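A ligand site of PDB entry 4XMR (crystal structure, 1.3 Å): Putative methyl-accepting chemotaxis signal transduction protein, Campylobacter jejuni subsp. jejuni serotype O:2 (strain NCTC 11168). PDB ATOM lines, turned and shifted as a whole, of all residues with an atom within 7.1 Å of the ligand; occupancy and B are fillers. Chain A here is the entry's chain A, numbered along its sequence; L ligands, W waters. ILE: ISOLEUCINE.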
ATOM      1  N   LEU A  79     -22.750  31.356 -13.528  1.00  0.00           N
ATOM      2  CA  LEU A  79     -22.461  29.969 -13.210  1.00  0.00           C
ATOM      3  C   LEU A  79     -22.961  29.591 -11.805  1.00  0.00           C
ATOM      4  O   LEU A  79     -23.583  28.540 -11.614  1.00  0.00           O
ATOM      5  CB  LEU A  79     -20.964  29.715 -13.300  1.00  0.00           C
ATOM      6  CG  LEU A  79     -20.561  28.241 -13.346  1.00  0.00           C
ATOM      7  CD1 LEU A  79     -21.037  27.618 -14.654  1.00  0.00           C
ATOM      8  CD2 LEU A  79     -19.061  28.074 -13.175  1.00  0.00           C
ATOM      9  N   ASN A  80     -22.670  30.462 -10.829  1.00  0.00           N
ATOM     10  CA  ASN A  80     -23.080  30.250  -9.445  1.00  0.00           C
ATOM     11  C   ASN A  80     -23.459  31.601  -8.890  1.00  0.00           C
ATOM     12  O   ASN A  80     -22.834  32.613  -9.199  1.00  0.00           O
ATOM     13  CB  ASN A  80     -21.918  29.730  -8.586  1.00  0.00           C
ATOM     14  CG  ASN A  80     -21.415  28.361  -8.989  1.00  0.00           C
ATOM     15  OD1 ASN A  80     -22.173  27.399  -9.033  1.00  0.00           O
ATOM     16  ND2 ASN A  80     -20.116  28.276  -9.271  1.00  0.00           N
ATOM     17  N   VAL A  81     -24.452  31.620  -8.001  1.00  0.00           N
ATOM     18  CA  VAL A  81     -24.819  32.818  -7.252  1.00  0.00           C
ATOM     19  C   VAL A  81     -25.104  32.327  -5.837  1.00  0.00           C
ATOM     20  O   VAL A  81     -25.814  31.330  -5.663  1.00  0.00           O
ATOM     21  CB  VAL A  81     -26.057  33.530  -7.868  1.00  0.00           C
ATOM     22  CG1 VAL A  81     -26.479  34.718  -7.007  1.00  0.00           C
ATOM     23  CG2 VAL A  81     -25.766  33.986  -9.287  1.00  0.00           C
ATOM     24  N   TYR A  82     -24.540  32.974  -4.828  1.00  0.00           N
ATOM     25  CA  TYR A  82     -24.550  32.398  -3.493  1.00  0.00           C
ATOM     26  C   TYR A  82     -24.436  33.433  -2.399  1.00  0.00           C
ATOM     27  O   TYR A  82     -23.999  34.570  -2.619  1.00  0.00           O
ATOM     28  CB  TYR A  82     -23.424  31.357  -3.368  1.00  0.00           C
ATOM     29  CG  TYR A  82     -22.068  31.778  -3.910  1.00  0.00           C
ATOM     30  CD1 TYR A  82     -21.747  31.577  -5.251  1.00  0.00           C
ATOM     31  CD2 TYR A  82     -21.103  32.363  -3.088  1.00  0.00           C
ATOM     32  CE1 TYR A  82     -20.511  31.940  -5.772  1.00  0.00           C
ATOM     33  CE2 TYR A  82     -19.856  32.723  -3.597  1.00  0.00           C
ATOM     34  CZ  TYR A  82     -19.564  32.507  -4.935  1.00  0.00           C
ATOM     35  OH  TYR A  82     -18.321  32.850  -5.417  1.00  0.00           O
ATOM     36  N   LEU A  83     -24.807  32.996  -1.185  1.00  0.00           N
ATOM     37  CA  LEU A  83     -24.711  33.837   0.009  1.00  0.00           C
ATOM     38  C   LEU A  83     -24.008  33.050   1.106  1.00  0.00           C
ATOM     39  O   LEU A  83     -24.533  32.038   1.587  1.00  0.00           O
ATOM     40  CB  LEU A  83     -26.108  34.282   0.463  1.00  0.00           C
ATOM     41  CG  LEU A  83     -26.124  35.197   1.701  1.00  0.00           C
ATOM     42  CD1 LEU A  83     -25.399  36.522   1.436  1.00  0.00           C
ATOM     43  CD2 LEU A  83     -27.540  35.447   2.214  1.00  0.00           C
ATOM     44  N   GLY A  84     -22.817  33.501   1.484  1.00  0.00           N
ATOM     45  CA  GLY A  84     -22.037  32.856   2.535  1.00  0.00           C
ATOM     46  C   GLY A  84     -22.266  33.460   3.903  1.00  0.00           C
ATOM     47  O   GLY A  84     -22.267  34.696   4.054  1.00  0.00           O
ATOM     48  N   VAL A  90     -22.917  28.104   3.113  1.00  0.00           N
ATOM     49  CA  VAL A  90     -23.201  28.969   1.977  1.00  0.00           C
ATOM     50  C   VAL A  90     -24.444  28.466   1.253  1.00  0.00           C
ATOM     51  O   VAL A  90     -24.555  27.261   0.965  1.00  0.00           O
ATOM     52  CB  VAL A  90     -21.981  29.107   1.018  1.00  0.00           C
ATOM     53  CG1 VAL A  90     -21.520  27.752   0.487  1.00  0.00           C
ATOM     54  CG2 VAL A  90     -22.295  30.053  -0.131  1.00  0.00           C
ATOM     55  N   LEU A  91     -25.383  29.366   1.005  1.00  0.00           N
ATOM     56  CA  LEU A  91     -26.554  29.040   0.198  1.00  0.00           C
ATOM     57  C   LEU A  91     -26.147  29.194  -1.268  1.00  0.00           C
ATOM     58  O   LEU A  91     -25.824  30.291  -1.719  1.00  0.00           O
ATOM     59  CB  LEU A  91     -27.702  29.981   0.526  1.00  0.00           C
ATOM     60  CG  LEU A  91     -28.973  29.713  -0.269  1.00  0.00           C
ATOM     61  CD1 LEU A  91     -29.543  28.327   0.044  1.00  0.00           C
ATOM     62  CD2 LEU A  91     -30.006  30.802  -0.031  1.00  0.00           C
ATOM     63  N   LEU A  92     -26.190  28.104  -2.020  1.00  0.00           N
ATOM     64  CA  LEU A  92     -25.626  28.062  -3.356  1.00  0.00           C
ATOM     65  C   LEU A  92     -26.679  27.750  -4.397  1.00  0.00           C
ATOM     66  O   LEU A  92     -27.358  26.727  -4.334  1.00  0.00           O
ATOM     67  CB  LEU A  92     -24.529  26.994  -3.414  1.00  0.00           C
ATOM     68  CG  LEU A  92     -23.918  26.693  -4.793  1.00  0.00           C
ATOM     69  CD1 LEU A  92     -23.323  27.949  -5.419  1.00  0.00           C
ATOM     70  CD2 LEU A  92     -22.889  25.589  -4.664  1.00  0.00           C
ATOM     71  N   ARG A 105     -24.749  24.585   1.789  1.00  0.00           N
ATOM     72  CA  ARG A 105     -23.571  23.715   1.775  1.00  0.00           C
ATOM     73  C   ARG A 105     -22.650  24.082   2.935  1.00  0.00           C
ATOM     74  O   ARG A 105     -22.389  25.251   3.172  1.00  0.00           O
ATOM     75  CB  ARG A 105     -22.792  23.917   0.462  1.00  0.00           C
ATOM     76  CG  ARG A 105     -23.557  23.601  -0.807  1.00  0.00           C
ATOM     77  CD  ARG A 105     -23.481  22.118  -1.127  1.00  0.00           C
ATOM     78  NE  ARG A 105     -22.116  21.616  -1.267  1.00  0.00           N
ATOM     79  CZ  ARG A 105     -21.496  21.410  -2.424  1.00  0.00           C
ATOM     80  NH1 ARG A 105     -22.127  21.659  -3.572  1.00  0.00           N
ATOM     81  NH2 ARG A 105     -20.258  20.940  -2.437  1.00  0.00           N
ATOM     82  N   LEU A 108     -17.653  23.958   1.797  1.00  0.00           N
ATOM     83  CA  LEU A 108     -16.939  24.760   0.813  1.00  0.00           C
ATOM     84  C   LEU A 108     -15.860  25.684   1.379  1.00  0.00           C
ATOM     85  O   LEU A 108     -15.295  26.513   0.650  1.00  0.00           O
ATOM     86  CB  LEU A 108     -17.924  25.502  -0.104  1.00  0.00           C
ATOM     87  CG  LEU A 108     -18.772  24.533  -0.955  1.00  0.00           C
ATOM     88  CD1 LEU A 108     -19.836  25.256  -1.746  1.00  0.00           C
ATOM     89  CD2 LEU A 108     -17.883  23.715  -1.894  1.00  0.00           C
ATOM     90  N   ASP A 109     -15.543  25.524   2.671  1.00  0.00           N
ATOM     91  CA  ASP A 109     -14.404  26.202   3.291  1.00  0.00           C
ATOM     92  C   ASP A 109     -14.400  27.702   3.001  1.00  0.00           C
ATOM     93  O   ASP A 109     -13.374  28.266   2.629  1.00  0.00           O
ATOM     94  CB  ASP A 109     -13.102  25.585   2.804  1.00  0.00           C
ATOM     95  CG  ASP A 109     -13.016  24.102   3.071  1.00  0.00           C
ATOM     96  OD1 ASP A 109     -13.303  23.703   4.222  1.00  0.00           O
ATOM     97  OD2 ASP A 109     -12.685  23.335   2.136  1.00  0.00           O
ATOM     98  N   ILE A 110     -15.548  28.352   3.171  1.00  0.00           N
ATOM     99  CA  ILE A 110     -15.700  29.689   2.613  1.00  0.00           C
ATOM    100  C   ILE A 110     -14.828  30.734   3.295  1.00  0.00           C
ATOM    101  O   ILE A 110     -14.379  31.674   2.646  1.00  0.00           O
ATOM    102  CB  ILE A 110     -17.152  30.148   2.537  1.00  0.00           C
ATOM    103  CG1 ILE A 110     -17.734  30.379   3.940  1.00  0.00           C
ATOM    104  CG2 ILE A 110     -17.984  29.139   1.754  1.00  0.00           C
ATOM    105  CD1 ILE A 110     -19.200  30.812   3.939  1.00  0.00           C
ATOM    106  N   LYS A 113     -11.578  31.543   1.641  1.00  0.00           N
ATOM    107  CA  LYS A 113     -11.657  32.035   0.257  1.00  0.00           C
ATOM    108  C   LYS A 113     -11.480  33.548   0.183  1.00  0.00           C
ATOM    109  O   LYS A 113     -12.034  34.295   0.994  1.00  0.00           O
ATOM    110  CB  LYS A 113     -13.004  31.656  -0.373  1.00  0.00           C
ATOM    111  CG  LYS A 113     -13.301  30.167  -0.389  1.00  0.00           C
ATOM    112  CD  LYS A 113     -12.414  29.443  -1.385  1.00  0.00           C
ATOM    113  CE  LYS A 113     -12.591  27.931  -1.312  1.00  0.00           C
ATOM    114  NZ  LYS A 113     -13.934  27.474  -1.768  1.00  0.00           N
ATOM    115  N   TRP A 115     -12.777  35.552  -1.988  1.00  0.00           N
ATOM    116  CA  TRP A 115     -14.031  36.251  -2.291  1.00  0.00           C
ATOM    117  C   TRP A 115     -14.783  36.582  -1.004  1.00  0.00           C
ATOM    118  O   TRP A 115     -15.444  37.609  -0.907  1.00  0.00           O
ATOM    119  CB  TRP A 115     -14.917  35.479  -3.292  1.00  0.00           C
ATOM    120  CG  TRP A 115     -15.412  34.137  -2.816  1.00  0.00           C
ATOM    121  CD1 TRP A 115     -14.904  32.923  -3.163  1.00  0.00           C
ATOM    122  CD2 TRP A 115     -16.516  33.873  -1.939  1.00  0.00           C
ATOM    123  NE1 TRP A 115     -15.616  31.915  -2.550  1.00  0.00           N
ATOM    124  CE2 TRP A 115     -16.609  32.482  -1.781  1.00  0.00           C
ATOM    125  CE3 TRP A 115     -17.445  34.693  -1.274  1.00  0.00           C
ATOM    126  CZ2 TRP A 115     -17.591  31.879  -0.987  1.00  0.00           C
ATOM    127  CZ3 TRP A 115     -18.419  34.098  -0.487  1.00  0.00           C
ATOM    128  CH2 TRP A 115     -18.473  32.701  -0.344  1.00  0.00           C
ATOM    129  N   TYR A 131     -10.136  32.203 -11.466  1.00  0.00           N
ATOM    130  CA  TYR A 131      -9.686  31.010 -10.763  1.00  0.00           C
ATOM    131  C   TYR A 131     -10.635  29.841 -11.057  1.00  0.00           C
ATOM    132  O   TYR A 131     -11.747  30.054 -11.564  1.00  0.00           O
ATOM    133  CB  TYR A 131      -9.589  31.263  -9.249  1.00  0.00           C
ATOM    134  CG  TYR A 131     -10.943  31.436  -8.614  1.00  0.00           C
ATOM    135  CD1 TYR A 131     -11.595  32.662  -8.649  1.00  0.00           C
ATOM    136  CD2 TYR A 131     -11.574  30.366  -7.985  1.00  0.00           C
ATOM    137  CE1 TYR A 131     -12.843  32.824  -8.090  1.00  0.00           C
ATOM    138  CE2 TYR A 131     -12.818  30.517  -7.407  1.00  0.00           C
ATOM    139  CZ  TYR A 131     -13.453  31.746  -7.459  1.00  0.00           C
ATOM    140  OH  TYR A 131     -14.699  31.895  -6.912  1.00  0.00           O
ATOM    141  N   LEU A 132     -10.199  28.632 -10.748  1.00  0.00           N
ATOM    142  CA  LEU A 132     -10.988  27.435 -11.019  1.00  0.00           C
ATOM    143  C   LEU A 132     -12.026  27.235  -9.915  1.00  0.00           C
ATOM    144  O   LEU A 132     -11.689  26.969  -8.769  1.00  0.00           O
ATOM    145  CB  LEU A 132     -10.081  26.214 -11.134  1.00  0.00           C
ATOM    146  CG  LEU A 132     -10.765  24.935 -11.625  1.00  0.00           C
ATOM    147  CD1 LEU A 132     -11.176  25.060 -13.093  1.00  0.00           C
ATOM    148  CD2 LEU A 132      -9.850  23.724 -11.440  1.00  0.00           C
ATOM    149  N   ASP A 133     -13.292  27.400 -10.282  1.00  0.00           N
ATOM    150  CA  ASP A 133     -14.401  27.228  -9.351  1.00  0.00           C
ATOM    151  C   ASP A 133     -14.389  25.829  -8.745  1.00  0.00           C
ATOM    152  O   ASP A 133     -14.236  24.842  -9.446  1.00  0.00           O
ATOM    153  CB  ASP A 133     -15.719  27.452 -10.087  1.00  0.00           C
ATOM    154  CG  ASP A 133     -16.926  27.021  -9.274  1.00  0.00           C
ATOM    155  OD1 ASP A 133     -16.954  27.265  -8.050  1.00  0.00           O
ATOM    156  OD2 ASP A 133     -17.849  26.437  -9.873  1.00  0.00           O
ATOM    157  N   THR A 134     -14.560  25.774  -7.428  1.00  0.00           N
ATOM    158  CA  THR A 134     -14.550  24.511  -6.688  1.00  0.00           C
ATOM    159  C   THR A 134     -15.675  23.586  -7.108  1.00  0.00           C
ATOM    160  O   THR A 134     -15.480  22.368  -7.212  1.00  0.00           O
ATOM    161  CB  THR A 134     -14.690  24.789  -5.170  1.00  0.00           C
ATOM    162  OG1 THR A 134     -13.654  25.670  -4.741  1.00  0.00           O
ATOM    163  CG2 THR A 134     -14.619  23.487  -4.374  1.00  0.00           C
ATOM    164  N   VAL A 135     -16.861  24.144  -7.339  1.00  0.00           N
ATOM    165  CA  VAL A 135     -18.042  23.305  -7.529  1.00  0.00           C
ATOM    166  C   VAL A 135     -18.202  22.788  -8.951  1.00  0.00           C
ATOM    167  O   VAL A 135     -18.461  21.608  -9.158  1.00  0.00           O
ATOM    168  CB  VAL A 135     -19.317  24.045  -7.049  1.00  0.00           C
ATOM    169  CG1 VAL A 135     -20.570  23.261  -7.438  1.00  0.00           C
ATOM    170  CG2 VAL A 135     -19.273  24.235  -5.533  1.00  0.00           C
ATOM    171  N   LEU A 136     -18.030  23.657  -9.936  1.00  0.00           N
ATOM    172  CA  LEU A 136     -18.253  23.272 -11.328  1.00  0.00           C
ATOM    173  C   LEU A 136     -16.989  23.165 -12.184  1.00  0.00           C
ATOM    174  O   LEU A 136     -17.060  22.815 -13.359  1.00  0.00           O
ATOM    175  CB  LEU A 136     -19.273  24.216 -11.983  1.00  0.00           C
ATOM    176  CG  LEU A 136     -20.691  24.066 -11.430  1.00  0.00           C
ATOM    177  CD1 LEU A 136     -21.643  25.089 -12.000  1.00  0.00           C
ATOM    178  CD2 LEU A 136     -21.204  22.662 -11.685  1.00  0.00           C
ATOM    179  N   GLN A 138     -14.952  25.237 -13.594  1.00  0.00           N
ATOM    180  CA  GLN A 138     -14.751  26.147 -14.702  1.00  0.00           C
ATOM    181  C   GLN A 138     -14.060  27.391 -14.174  1.00  0.00           C
ATOM    182  O   GLN A 138     -14.231  27.746 -13.008  1.00  0.00           O
ATOM    183  CB  GLN A 138     -16.084  26.535 -15.343  1.00  0.00           C
ATOM    184  CG  GLN A 138     -16.792  25.370 -16.006  1.00  0.00           C
ATOM    185  CD  GLN A 138     -18.112  25.784 -16.631  1.00  0.00           C
ATOM    186  OE1 GLN A 138     -18.219  26.860 -17.222  1.00  0.00           O
ATOM    187  NE2 GLN A 138     -19.118  24.935 -16.495  1.00  0.00           N
ATOM    188  N   VAL A 140     -13.653  31.076 -13.387  1.00  0.00           N
ATOM    189  CA  VAL A 140     -14.596  32.140 -13.138  1.00  0.00           C
ATOM    190  C   VAL A 140     -13.939  33.394 -12.625  1.00  0.00           C
ATOM    191  O   VAL A 140     -12.839  33.348 -12.042  1.00  0.00           O
ATOM    192  CB  VAL A 140     -15.673  31.710 -12.118  1.00  0.00           C
ATOM    193  CG1 VAL A 140     -16.442  30.515 -12.631  1.00  0.00           C
ATOM    194  CG2 VAL A 140     -15.054  31.437 -10.729  1.00  0.00           C
ATOM    195  N   THR A 142     -15.162  36.135  -9.864  1.00  0.00           N
ATOM    196  CA  THR A 142     -16.162  36.272  -8.815  1.00  0.00           C
ATOM    197  C   THR A 142     -16.314  37.725  -8.389  1.00  0.00           C
ATOM    198  O   THR A 142     -15.325  38.425  -8.161  1.00  0.00           O
ATOM    199  CB  THR A 142     -15.820  35.394  -7.598  1.00  0.00           C
ATOM    200  OG1 THR A 142     -15.857  34.011  -7.994  1.00  0.00           O
ATOM    201  CG2 THR A 142     -16.794  35.640  -6.424  1.00  0.00           C
ATOM    202  N   ASP A 160     -20.461  34.198  -9.642  1.00  0.00           N
ATOM    203  CA  ASP A 160     -19.411  33.642 -10.492  1.00  0.00           C
ATOM    204  C   ASP A 160     -19.809  33.751 -11.960  1.00  0.00           C
ATOM    205  O   ASP A 160     -20.808  33.178 -12.396  1.00  0.00           O
ATOM    206  CB  ASP A 160     -19.137  32.158 -10.193  1.00  0.00           C
ATOM    207  CG  ASP A 160     -18.627  31.906  -8.789  1.00  0.00           C
ATOM    208  OD1 ASP A 160     -18.200  32.849  -8.096  1.00  0.00           O
ATOM    209  OD2 ASP A 160     -18.642  30.713  -8.402  1.00  0.00           O
HETATM  210  N   ILE L   1     -16.623  29.811  -6.797  1.00  0.00           N
HETATM  211  CA  ILE L   1     -16.708  29.768  -5.340  1.00  0.00           C
HETATM  212  C   ILE L   1     -15.507  29.007  -4.820  1.00  0.00           C
HETATM  213  O   ILE L   1     -14.869  28.257  -5.576  1.00  0.00           O
HETATM  214  CB  ILE L   1     -18.035  29.126  -4.858  1.00  0.00           C
HETATM  215  CG1 ILE L   1     -18.295  29.442  -3.386  1.00  0.00           C
HETATM  216  CG2 ILE L   1     -18.039  27.624  -5.092  1.00  0.00           C
HETATM  217  CD1 ILE L   1     -19.662  29.037  -2.945  1.00  0.00           C
HETATM  218  OXT ILE L   1     -15.155  29.154  -3.659  1.00  0.00           O
HETATM  219  O   HOH W   1     -12.074  28.326  -4.498  1.00  0.00           O
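The side-chain carboxylate (OD2) of Asp 160 lies within salt-bridge range of a nitrogen (N) of the ligand. The side-chain amino group of Lys 113 is in salt-bridge range of an oxygen (OXT) of the ligand. A nitrogen (N) of the ligand is in hydrogen-bond range of the side-chain hydroxyl of Tyr 131. OD1 of Asp 133 is in salt-bridge range of N of the ligand (2.9 Å). An oxygen (O) of the ligand is in hydrogen-bond range of the backbone NH (N) of Thr 134 (3.1 Å). An oxygen (O) of the ligand lies within hydrogen-bond range of the side-chain hydroxyl (OG1) of Thr 134 (3.0 Å). The indole nitrogen (NE1) of Trp 115 sits at hydrogen-bond distance from an oxygen (OXT) of the ligand, 3.0 Å away.
Water W1 lies within hydrogen-bond range of O of the ligand (3.0 Å), OG1 of Thr 134 (3.1 Å) and NZ of Lys 113 (3.4 Å).
OD1 of Asp 160 is in hydrogen-bond range of OG1 of Thr 142, 2.6 Å away. N of Asp 160 sits at hydrogen-bond distance from O of Asn 80, 2.9 Å away. O of Asp 160 is in hydrogen-bond range of N of Leu 79 (2.9 Å). O of Leu 108 sits at hydrogen-bond distance from NZ of Lys 113, 2.9 Å away. The side-chain carboxylate of Asp 133 is in hydrogen-bond range of the backbone NH of Val 135 (3.2 Å). OD2 of Asp 133 lies within hydrogen-bond range of ND2 of Asn 80 (3.0 Å). The side-chain carboxylate (OD2) of Asp 133 lies within hydrogen-bond range of the backbone NH (N) of Leu 136 (2.8 Å). O of Val 90 sits at hydrogen-bond distance from N of Arg 105.
Merely in contact with the ligand: Tyr 82 (3.5 Å), Val 90 (3.99 Å), Leu 108 (3.97 Å) and Val 135 (3.6 Å). Hydrophobic or aromatic side chains that line the ligand: Tyr 82, Val 90, Leu 108, Trp 115, Tyr 131 and Val 135. The nearest printed residue that does not touch the ligand is Thr 142 (4.4 Å).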
